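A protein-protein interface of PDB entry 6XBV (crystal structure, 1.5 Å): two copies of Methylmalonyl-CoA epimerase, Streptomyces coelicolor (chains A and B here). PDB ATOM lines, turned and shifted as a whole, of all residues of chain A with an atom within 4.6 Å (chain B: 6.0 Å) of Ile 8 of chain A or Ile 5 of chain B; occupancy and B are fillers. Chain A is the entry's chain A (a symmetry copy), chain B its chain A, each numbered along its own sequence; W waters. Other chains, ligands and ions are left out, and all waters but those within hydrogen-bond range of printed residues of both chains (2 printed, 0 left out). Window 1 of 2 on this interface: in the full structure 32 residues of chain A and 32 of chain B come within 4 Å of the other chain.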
ATOM      1  N   HIS A   7      11.995  28.375 -20.081  1.00  0.00           N
ATOM      2  CA  HIS A   7      12.080  29.701 -20.709  1.00  0.00           C
ATOM      3  C   HIS A   7      13.367  29.800 -21.516  1.00  0.00           C
ATOM      4  O   HIS A   7      14.336  29.052 -21.327  1.00  0.00           O
ATOM      5  CB  HIS A   7      11.921  30.861 -19.745  1.00  0.00           C
ATOM      6  CG  HIS A   7      12.950  30.949 -18.639  1.00  0.00           C
ATOM      7  ND1 HIS A   7      12.736  30.316 -17.384  1.00  0.00           N
ATOM      8  CD2 HIS A   7      14.091  31.678 -18.546  1.00  0.00           C
ATOM      9  CE1 HIS A   7      13.762  30.727 -16.619  1.00  0.00           C
ATOM     10  NE2 HIS A   7      14.625  31.524 -17.271  1.00  0.00           N
ATOM     11  N   ILE A   8      13.372  30.828 -22.375  1.00  0.00           N
ATOM     12  CA  ILE A   8      14.578  31.301 -23.108  1.00  0.00           C
ATOM     13  C   ILE A   8      14.942  32.662 -22.510  1.00  0.00           C
ATOM     14  O   ILE A   8      14.056  33.545 -22.527  1.00  0.00           O
ATOM     15  CB  ILE A   8      14.336  31.396 -24.621  1.00  0.00           C
ATOM     16  CG1 ILE A   8      13.833  30.054 -25.166  1.00  0.00           C
ATOM     17  CG2 ILE A   8      15.637  31.829 -25.322  1.00  0.00           C
ATOM     18  CD1 ILE A   8      13.291  30.067 -26.580  1.00  0.00           C
ATOM     19  N   GLY A   9      16.138  32.805 -21.965  1.00  0.00           N
ATOM     20  CA  GLY A   9      16.598  34.087 -21.432  1.00  0.00           C
ATOM     21  C   GLY A   9      17.238  34.931 -22.489  1.00  0.00           C
ATOM     22  O   GLY A   9      18.224  34.468 -23.089  1.00  0.00           O
ATOM     23  N   ILE A  10      16.678  36.066 -22.793  1.00  0.00           N
ATOM     24  CA  ILE A  10      17.074  36.962 -23.905  1.00  0.00           C
ATOM     25  C   ILE A  10      17.523  38.276 -23.296  1.00  0.00           C
ATOM     26  O   ILE A  10      16.710  38.940 -22.630  1.00  0.00           O
ATOM     27  CB  ILE A  10      15.898  37.153 -24.871  1.00  0.00           C
ATOM     28  CG1 ILE A  10      15.546  35.805 -25.531  1.00  0.00           C
ATOM     29  CG2 ILE A  10      16.232  38.232 -25.888  1.00  0.00           C
ATOM     30  CD1 ILE A  10      14.301  35.789 -26.318  1.00  0.00           C
ATOM     31  N   ILE A  48       4.338  31.893 -23.817  1.00  0.00           N
ATOM     32  CA  ILE A  48       4.077  31.457 -25.186  1.00  0.00           C
ATOM     33  C   ILE A  48       3.144  30.278 -25.231  1.00  0.00           C
ATOM     34  O   ILE A  48       2.301  30.251 -26.143  1.00  0.00           O
ATOM     35  CB  ILE A  48       5.435  31.196 -25.890  1.00  0.00           C
ATOM     36  CG1 ILE A  48       6.456  32.316 -25.639  1.00  0.00           C
ATOM     37  CG2 ILE A  48       5.211  30.987 -27.384  1.00  0.00           C
ATOM     38  CD1 ILE A  48       5.985  33.685 -26.020  1.00  0.00           C
ATOM     39  N   ASN A  49       3.232  29.326 -24.289  1.00  0.00           N
ATOM     40  CA  ASN A  49       2.403  28.123 -24.340  1.00  0.00           C
ATOM     41  C   ASN A  49       2.403  27.497 -22.960  1.00  0.00           C
ATOM     42  O   ASN A  49       3.314  27.739 -22.140  1.00  0.00           O
ATOM     43  CB  ASN A  49       2.803  27.166 -25.429  1.00  0.00           C
ATOM     44  CG  ASN A  49       4.258  26.712 -25.353  1.00  0.00           C
ATOM     45  OD1 ASN A  49       5.104  27.351 -25.986  1.00  0.00           O
ATOM     46  ND2 ASN A  49       4.564  25.647 -24.620  1.00  0.00           N
ATOM     47  N   SER A  57       5.920  27.658 -20.834  1.00  0.00           N
ATOM     48  CA  SER A  57       7.156  28.096 -21.529  1.00  0.00           C
ATOM     49  C   SER A  57       7.045  29.562 -21.821  1.00  0.00           C
ATOM     50  O   SER A  57       6.009  30.005 -22.344  1.00  0.00           O
ATOM     51  CB  SER A  57       7.471  27.384 -22.819  1.00  0.00           C
ATOM     52  OG  SER A  57       7.726  25.985 -22.660  1.00  0.00           O
ATOM     53  N   TYR A  58       8.093  30.308 -21.494  1.00  0.00           N
ATOM     54  CA  TYR A  58       8.148  31.756 -21.563  1.00  0.00           C
ATOM     55  C   TYR A  58       9.345  32.238 -22.373  1.00  0.00           C
ATOM     56  O   TYR A  58      10.381  31.522 -22.438  1.00  0.00           O
ATOM     57  CB  TYR A  58       8.220  32.396 -20.173  1.00  0.00           C
ATOM     58  CG  TYR A  58       7.190  31.957 -19.158  1.00  0.00           C
ATOM     59  CD1 TYR A  58       7.352  30.795 -18.428  1.00  0.00           C
ATOM     60  CD2 TYR A  58       6.049  32.710 -18.933  1.00  0.00           C
ATOM     61  CE1 TYR A  58       6.461  30.421 -17.431  1.00  0.00           C
ATOM     62  CE2 TYR A  58       5.141  32.317 -17.959  1.00  0.00           C
ATOM     63  CZ  TYR A  58       5.356  31.206 -17.228  1.00  0.00           C
ATOM     64  OH  TYR A  58       4.450  30.821 -16.251  1.00  0.00           O
ATOM     65  N   LEU A  59       9.240  33.467 -22.855  1.00  0.00           N
ATOM     66  CA  LEU A  59      10.433  34.280 -23.157  1.00  0.00           C
ATOM     67  C   LEU A  59      10.709  35.126 -21.944  1.00  0.00           C
ATOM     68  O   LEU A  59       9.778  35.812 -21.440  1.00  0.00           O
ATOM     69  CB  LEU A  59      10.213  35.156 -24.384  1.00  0.00           C
ATOM     70  CG  LEU A  59       9.794  34.379 -25.611  1.00  0.00           C
ATOM     71  CD1 LEU A  59       9.542  35.396 -26.735  1.00  0.00           C
ATOM     72  CD2 LEU A  59      10.820  33.382 -26.070  1.00  0.00           C
ATOM     73  N   GLN A  60      11.935  35.070 -21.404  1.00  0.00           N
ATOM     74  CA  GLN A  60      12.368  35.906 -20.266  1.00  0.00           C
ATOM     75  C   GLN A  60      13.265  36.986 -20.845  1.00  0.00           C
ATOM     76  O   GLN A  60      14.435  36.712 -21.188  1.00  0.00           O
ATOM     77  CB  GLN A  60      13.052  35.048 -19.226  1.00  0.00           C
ATOM     78  CG  GLN A  60      13.592  35.865 -18.065  1.00  0.00           C
ATOM     79  CD  GLN A  60      14.250  34.997 -17.040  1.00  0.00           C
ATOM     80  OE1 GLN A  60      15.286  34.436 -17.320  1.00  0.00           O
ATOM     81  NE2 GLN A  60      13.581  34.833 -15.901  1.00  0.00           N
ATOM     82  N   VAL A  82      20.279  35.902 -27.302  1.00  0.00           N
ATOM     83  CA  VAL A  82      20.022  34.811 -26.343  1.00  0.00           C
ATOM     84  C   VAL A  82      21.162  34.699 -25.340  1.00  0.00           C
ATOM     85  O   VAL A  82      22.321  34.462 -25.751  1.00  0.00           O
ATOM     86  CB  VAL A  82      19.710  33.492 -27.053  1.00  0.00           C
ATOM     87  CG1 VAL A  82      19.473  32.386 -26.030  1.00  0.00           C
ATOM     88  CG2 VAL A  82      18.526  33.562 -27.992  1.00  0.00           C
ATOM     89  N   HIS A  84      20.611  32.629 -22.120  1.00  0.00           N
ATOM     90  CA  HIS A  84      20.577  31.332 -21.422  1.00  0.00           C
ATOM     91  C   HIS A  84      19.340  30.555 -21.819  1.00  0.00           C
ATOM     92  O   HIS A  84      18.412  31.180 -22.381  1.00  0.00           O
ATOM     93  CB  HIS A  84      20.700  31.431 -19.902  1.00  0.00           C
ATOM     94  CG  HIS A  84      19.558  32.096 -19.207  1.00  0.00           C
ATOM     95  ND1 HIS A  84      19.554  33.469 -18.961  1.00  0.00           N
ATOM     96  CD2 HIS A  84      18.477  31.583 -18.546  1.00  0.00           C
ATOM     97  CE1 HIS A  84      18.451  33.743 -18.226  1.00  0.00           C
ATOM     98  NE2 HIS A  84      17.770  32.616 -17.928  1.00  0.00           N
ATOM     99  N   THR B   3       2.018  30.071 -31.670  1.00  0.00           N
ATOM    100  CA  THR B   3       1.337  29.407 -30.555  1.00  0.00           C
ATOM    101  C   THR B   3       2.253  28.563 -29.679  1.00  0.00           C
ATOM    102  O   THR B   3       1.761  28.041 -28.641  1.00  0.00           O
ATOM    103  CB  THR B   3       0.188  28.567 -31.100  1.00  0.00           C
ATOM    104  OG1 THR B   3       0.635  27.636 -32.074  1.00  0.00           O
ATOM    105  CG2 THR B   3      -0.867  29.492 -31.659  1.00  0.00           C
ATOM    106  N   ARG B   4       3.540  28.395 -29.998  1.00  0.00           N
ATOM    107  CA  ARG B   4       4.449  27.647 -29.118  1.00  0.00           C
ATOM    108  C   ARG B   4       5.877  28.081 -29.419  1.00  0.00           C
ATOM    109  O   ARG B   4       6.210  28.591 -30.520  1.00  0.00           O
ATOM    110  CB  ARG B   4       4.356  26.140 -29.329  1.00  0.00           C
ATOM    111  CG  ARG B   4       4.835  25.647 -30.662  1.00  0.00           C
ATOM    112  CD  ARG B   4       4.717  24.138 -30.837  1.00  0.00           C
ATOM    113  NE  ARG B   4       5.115  23.716 -32.151  1.00  0.00           N
ATOM    114  CZ  ARG B   4       4.348  23.818 -33.261  1.00  0.00           C
ATOM    115  NH1 ARG B   4       3.107  24.215 -33.164  1.00  0.00           N
ATOM    116  NH2 ARG B   4       4.864  23.545 -34.436  1.00  0.00           N
ATOM    117  N   ILE B   5       6.749  27.800 -28.435  1.00  0.00           N
ATOM    118  CA  ILE B   5       8.184  27.634 -28.751  1.00  0.00           C
ATOM    119  C   ILE B   5       8.313  26.250 -29.385  1.00  0.00           C
ATOM    120  O   ILE B   5       8.079  25.206 -28.692  1.00  0.00           O
ATOM    121  CB  ILE B   5       9.016  27.805 -27.487  1.00  0.00           C
ATOM    122  CG1 ILE B   5       8.851  29.209 -26.914  1.00  0.00           C
ATOM    123  CG2 ILE B   5      10.463  27.449 -27.800  1.00  0.00           C
ATOM    124  CD1 ILE B   5       9.518  29.520 -25.578  1.00  0.00           C
ATOM    125  N   ASP B   6       8.705  26.145 -30.635  1.00  0.00           N
ATOM    126  CA  ASP B   6       8.888  24.862 -31.322  1.00  0.00           C
ATOM    127  C   ASP B   6      10.262  24.284 -30.966  1.00  0.00           C
ATOM    128  O   ASP B   6      10.364  23.102 -30.653  1.00  0.00           O
ATOM    129  CB  ASP B   6       8.702  24.985 -32.830  1.00  0.00           C
ATOM    130  CG  ASP B   6       8.719  23.636 -33.511  1.00  0.00           C
ATOM    131  OD1 ASP B   6       7.587  22.984 -33.547  1.00  0.00           O
ATOM    132  OD2 ASP B   6       9.802  23.186 -34.002  1.00  0.00           O
ATOM    133  N   HIS B   7      11.330  25.062 -31.034  1.00  0.00           N
ATOM    134  CA  HIS B   7      12.644  24.485 -30.717  1.00  0.00           C
ATOM    135  C   HIS B   7      13.631  25.605 -30.417  1.00  0.00           C
ATOM    136  O   HIS B   7      13.450  26.774 -30.782  1.00  0.00           O
ATOM    137  CB  HIS B   7      13.173  23.523 -31.764  1.00  0.00           C
ATOM    138  CG  HIS B   7      13.386  24.100 -33.147  1.00  0.00           C
ATOM    139  ND1 HIS B   7      12.354  24.067 -34.124  1.00  0.00           N
ATOM    140  CD2 HIS B   7      14.506  24.582 -33.743  1.00  0.00           C
ATOM    141  CE1 HIS B   7      12.939  24.517 -35.248  1.00  0.00           C
ATOM    142  NE2 HIS B   7      14.223  24.870 -35.074  1.00  0.00           N
ATOM    143  N   ILE B   8      14.744  25.174 -29.807  1.00  0.00           N
ATOM    144  CA  ILE B   8      15.966  26.001 -29.615  1.00  0.00           C
ATOM    145  C   ILE B   8      17.038  25.409 -30.533  1.00  0.00           C
ATOM    146  O   ILE B   8      17.312  24.199 -30.379  1.00  0.00           O
ATOM    147  CB  ILE B   8      16.427  26.024 -28.150  1.00  0.00           C
ATOM    148  CG1 ILE B   8      15.283  26.484 -27.239  1.00  0.00           C
ATOM    149  CG2 ILE B   8      17.654  26.944 -28.012  1.00  0.00           C
ATOM    150  CD1 ILE B   8      15.495  26.294 -25.751  1.00  0.00           C
ATOM    151  N   THR B  51       3.187  20.481 -26.145  1.00  0.00           N
ATOM    152  CA  THR B  51       2.678  21.845 -25.911  1.00  0.00           C
ATOM    153  C   THR B  51       1.145  21.955 -26.126  1.00  0.00           C
ATOM    154  O   THR B  51       0.534  21.060 -26.775  1.00  0.00           O
ATOM    155  CB  THR B  51       3.429  22.814 -26.848  1.00  0.00           C
ATOM    156  OG1 THR B  51       3.245  22.453 -28.199  1.00  0.00           O
ATOM    157  CG2 THR B  51       4.920  22.888 -26.572  1.00  0.00           C
ATOM    158  N   ALA B  56       4.912  20.302 -30.054  1.00  0.00           N
ATOM    159  CA  ALA B  56       5.970  19.870 -29.142  1.00  0.00           C
ATOM    160  C   ALA B  56       7.100  20.881 -29.162  1.00  0.00           C
ATOM    161  O   ALA B  56       7.174  21.735 -30.068  1.00  0.00           O
ATOM    162  CB  ALA B  56       6.448  18.509 -29.495  1.00  0.00           C
ATOM    163  N   SER B  57       7.988  20.737 -28.184  1.00  0.00           N
ATOM    164  CA  SER B  57       9.185  21.602 -28.031  1.00  0.00           C
ATOM    165  C   SER B  57      10.402  20.728 -27.985  1.00  0.00           C
ATOM    166  O   SER B  57      10.417  19.739 -27.235  1.00  0.00           O
ATOM    167  CB  SER B  57       9.201  22.491 -26.815  1.00  0.00           C
ATOM    168  OG  SER B  57       8.154  23.466 -26.797  1.00  0.00           O
ATOM    169  N   TYR B  58      11.411  21.084 -28.770  1.00  0.00           N
ATOM    170  CA  TYR B  58      12.622  20.314 -28.984  1.00  0.00           C
ATOM    171  C   TYR B  58      13.873  21.141 -28.718  1.00  0.00           C
ATOM    172  O   TYR B  58      13.835  22.393 -28.875  1.00  0.00           O
ATOM    173  CB  TYR B  58      12.708  19.758 -30.408  1.00  0.00           C
ATOM    174  CG  TYR B  58      11.505  19.002 -30.927  1.00  0.00           C
ATOM    175  CD1 TYR B  58      10.412  19.665 -31.449  1.00  0.00           C
ATOM    176  CD2 TYR B  58      11.467  17.617 -30.889  1.00  0.00           C
ATOM    177  CE1 TYR B  58       9.337  18.986 -32.008  1.00  0.00           C
ATOM    178  CE2 TYR B  58      10.377  16.941 -31.418  1.00  0.00           C
ATOM    179  CZ  TYR B  58       9.349  17.617 -31.968  1.00  0.00           C
ATOM    180  OH  TYR B  58       8.266  16.936 -32.501  1.00  0.00           O
ATOM    181  N   ILE B  85      16.144  30.651 -32.303  1.00  0.00           N
ATOM    182  CA  ILE B  85      14.938  30.166 -31.600  1.00  0.00           C
ATOM    183  C   ILE B  85      13.859  30.008 -32.638  1.00  0.00           C
ATOM    184  O   ILE B  85      13.850  30.739 -33.650  1.00  0.00           O
ATOM    185  CB  ILE B  85      14.554  31.046 -30.435  1.00  0.00           C
ATOM    186  CG1 ILE B  85      14.019  32.352 -30.904  1.00  0.00           C
ATOM    187  CG2 ILE B  85      15.726  31.252 -29.505  1.00  0.00           C
ATOM    188  CD1 ILE B  85      13.410  33.165 -29.736  1.00  0.00           C
ATOM    189  N   ALA B  86      12.953  29.062 -32.498  1.00  0.00           N
ATOM    190  CA  ALA B  86      11.884  28.810 -33.474  1.00  0.00           C
ATOM    191  C   ALA B  86      10.522  28.834 -32.787  1.00  0.00           C
ATOM    192  O   ALA B  86      10.342  28.128 -31.748  1.00  0.00           O
ATOM    193  CB  ALA B  86      12.114  27.478 -34.143  1.00  0.00           C
ATOM    194  N   PHE B  87       9.561  29.522 -33.388  1.00  0.00           N
ATOM    195  CA  PHE B  87       8.158  29.606 -32.954  1.00  0.00           C
ATOM    196  C   PHE B  87       7.317  28.779 -33.936  1.00  0.00           C
ATOM    197  O   PHE B  87       7.447  28.872 -35.132  1.00  0.00           O
ATOM    198  CB  PHE B  87       7.701  31.056 -32.914  1.00  0.00           C
ATOM    199  CG  PHE B  87       8.424  31.886 -31.891  1.00  0.00           C
ATOM    200  CD1 PHE B  87       8.228  31.735 -30.548  1.00  0.00           C
ATOM    201  CD2 PHE B  87       9.254  32.873 -32.278  1.00  0.00           C
ATOM    202  CE1 PHE B  87       8.953  32.474 -29.614  1.00  0.00           C
ATOM    203  CE2 PHE B  87       9.930  33.665 -31.355  1.00  0.00           C
ATOM    204  CZ  PHE B  87       9.818  33.420 -30.016  1.00  0.00           C
ATOM    205  N   GLY B  88       6.433  27.972 -33.365  1.00  0.00           N
ATOM    206  CA  GLY B  88       5.485  27.226 -34.205  1.00  0.00           C
ATOM    207  C   GLY B  88       4.171  27.946 -34.438  1.00  0.00           C
ATOM    208  O   GLY B  88       3.717  28.781 -33.607  1.00  0.00           O
HETATM  209  O   HOH W   1      -0.492  28.907 -27.253  1.00  0.00           O
HETATM  210  O   HOH W   2       7.196  24.327 -24.563  1.00  0.00           O
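The backbone carbonyl oxygen (O) of Thr 3 of chain B sits close to the backbone carbonyl oxygen (O) of Ile 48 of chain A, at 3.4 Å.
The backbone NH of Ile 5 of chain B is in hydrogen-bond range of the side-chain amide oxygen of Asn 49 of chain A (3.0 Å).
N of Ile 8 of chain A is in hydrogen-bond range of O of Tyr 58 of chain A (3.1 Å).
The backbone carbonyl oxygen of Asn 49 of chain A is in hydrogen-bond range of the backbone NH of Ser 57 of chain A (2.9 Å).
NH2 of Arg 4 of chain B lies within salt-bridge range of OD1 of Asp 6 of chain B, 2.9 Å away.
O of Gly 88 of chain B is in hydrogen-bond range of N of Thr 3 of chain B, 2.9 Å away.
The backbone carbonyl oxygen of Ile 5 of chain B lies within hydrogen-bond range of the side-chain hydroxyl of Ser 57 of chain B, at 2.6 Å.
The backbone carbonyl oxygen of Arg 4 of chain B sits at hydrogen-bond distance from the backbone NH of Gly 88 of chain B (2.9 Å).
Among the printed residues, pairs that only touch across the chains: Asn 49 of chain A with Arg 4 of chain B (3.2 Å), Asn 49 of chain A with Thr 51 of chain B (3.4 Å), Asn 49 of chain A with Thr 3 of chain B (3.5 Å), Ile 48 of chain A with Arg 4 of chain B (3.6 Å), Ile 48 of chain A with Ile 5 of chain B (3.7 Å), Tyr 58 of chain A with Ile 5 of chain B (3.8 Å), Leu 59 of chain A with Phe 87 of chain B (3.8 Å), Val 82 of chain A with Ile 85 of chain B (3.9 Å), Ile 8 of chain A with Ile 5 of chain B (3.9 Å) and Ile 8 of chain A with Ile 85 of chain B (3.99 Å).
Of the printed residues of chain B, Ile 8 of chain A touches Ile 5 and Ile 85.
Printed residues of chain A within 4 Å of Ile 5 of chain B: Ile 8 (3.9 Å), Ile 48 (3.7 Å), Asn 49 (3.0 Å) and Tyr 58 (3.8 Å).
Printed residues of chain B within 4 Å of Asn 49 of chain A: Thr 3, Arg 4, Ile 5 and Thr 51.
Of the printed residues of chain B, Leu 59 of chain A touches Phe 87.
Gln 60 of chain A touches none of the printed residues of chain B.
His 7 of chain A touches none of the printed residues of chain B.
The nearest printed residue of chain A that does not touch Ile 5 of chain B is Ser 57 of chain A (4.05 Å).
Printed residues of chain B that touch a printed residue of chain A: Thr 3, Arg 4, Ile 5, Thr 51, Ile 85 and Phe 87.
Among the printed residues, 12 pairs touch across the chains.
Among the printed residues, no Asp or Glu carboxylate lies within 4 Å of a Lys or Arg side-chain nitrogen of the other chain.
Positions printed for both chains: 7, 8, 57 and 58.
Of the 12 pairs that touch across the chains among the printed residues, none has its exchanged pair printed and touching as well.
Water W2 lies within hydrogen-bond range of the side-chain hydroxyl (OG) of Ser 57 of chain B (2.6 Å), the side-chain hydroxyl (OG) of Ser 57 of chain A (2.6 Å) and the side-chain amide nitrogen (ND2) of Asn 49 of chain A (2.9 Å).
Water W1 bridges O of Thr 3 of chain B (2.8 Å) and O of Ile 48 of chain A (3.3 Å).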
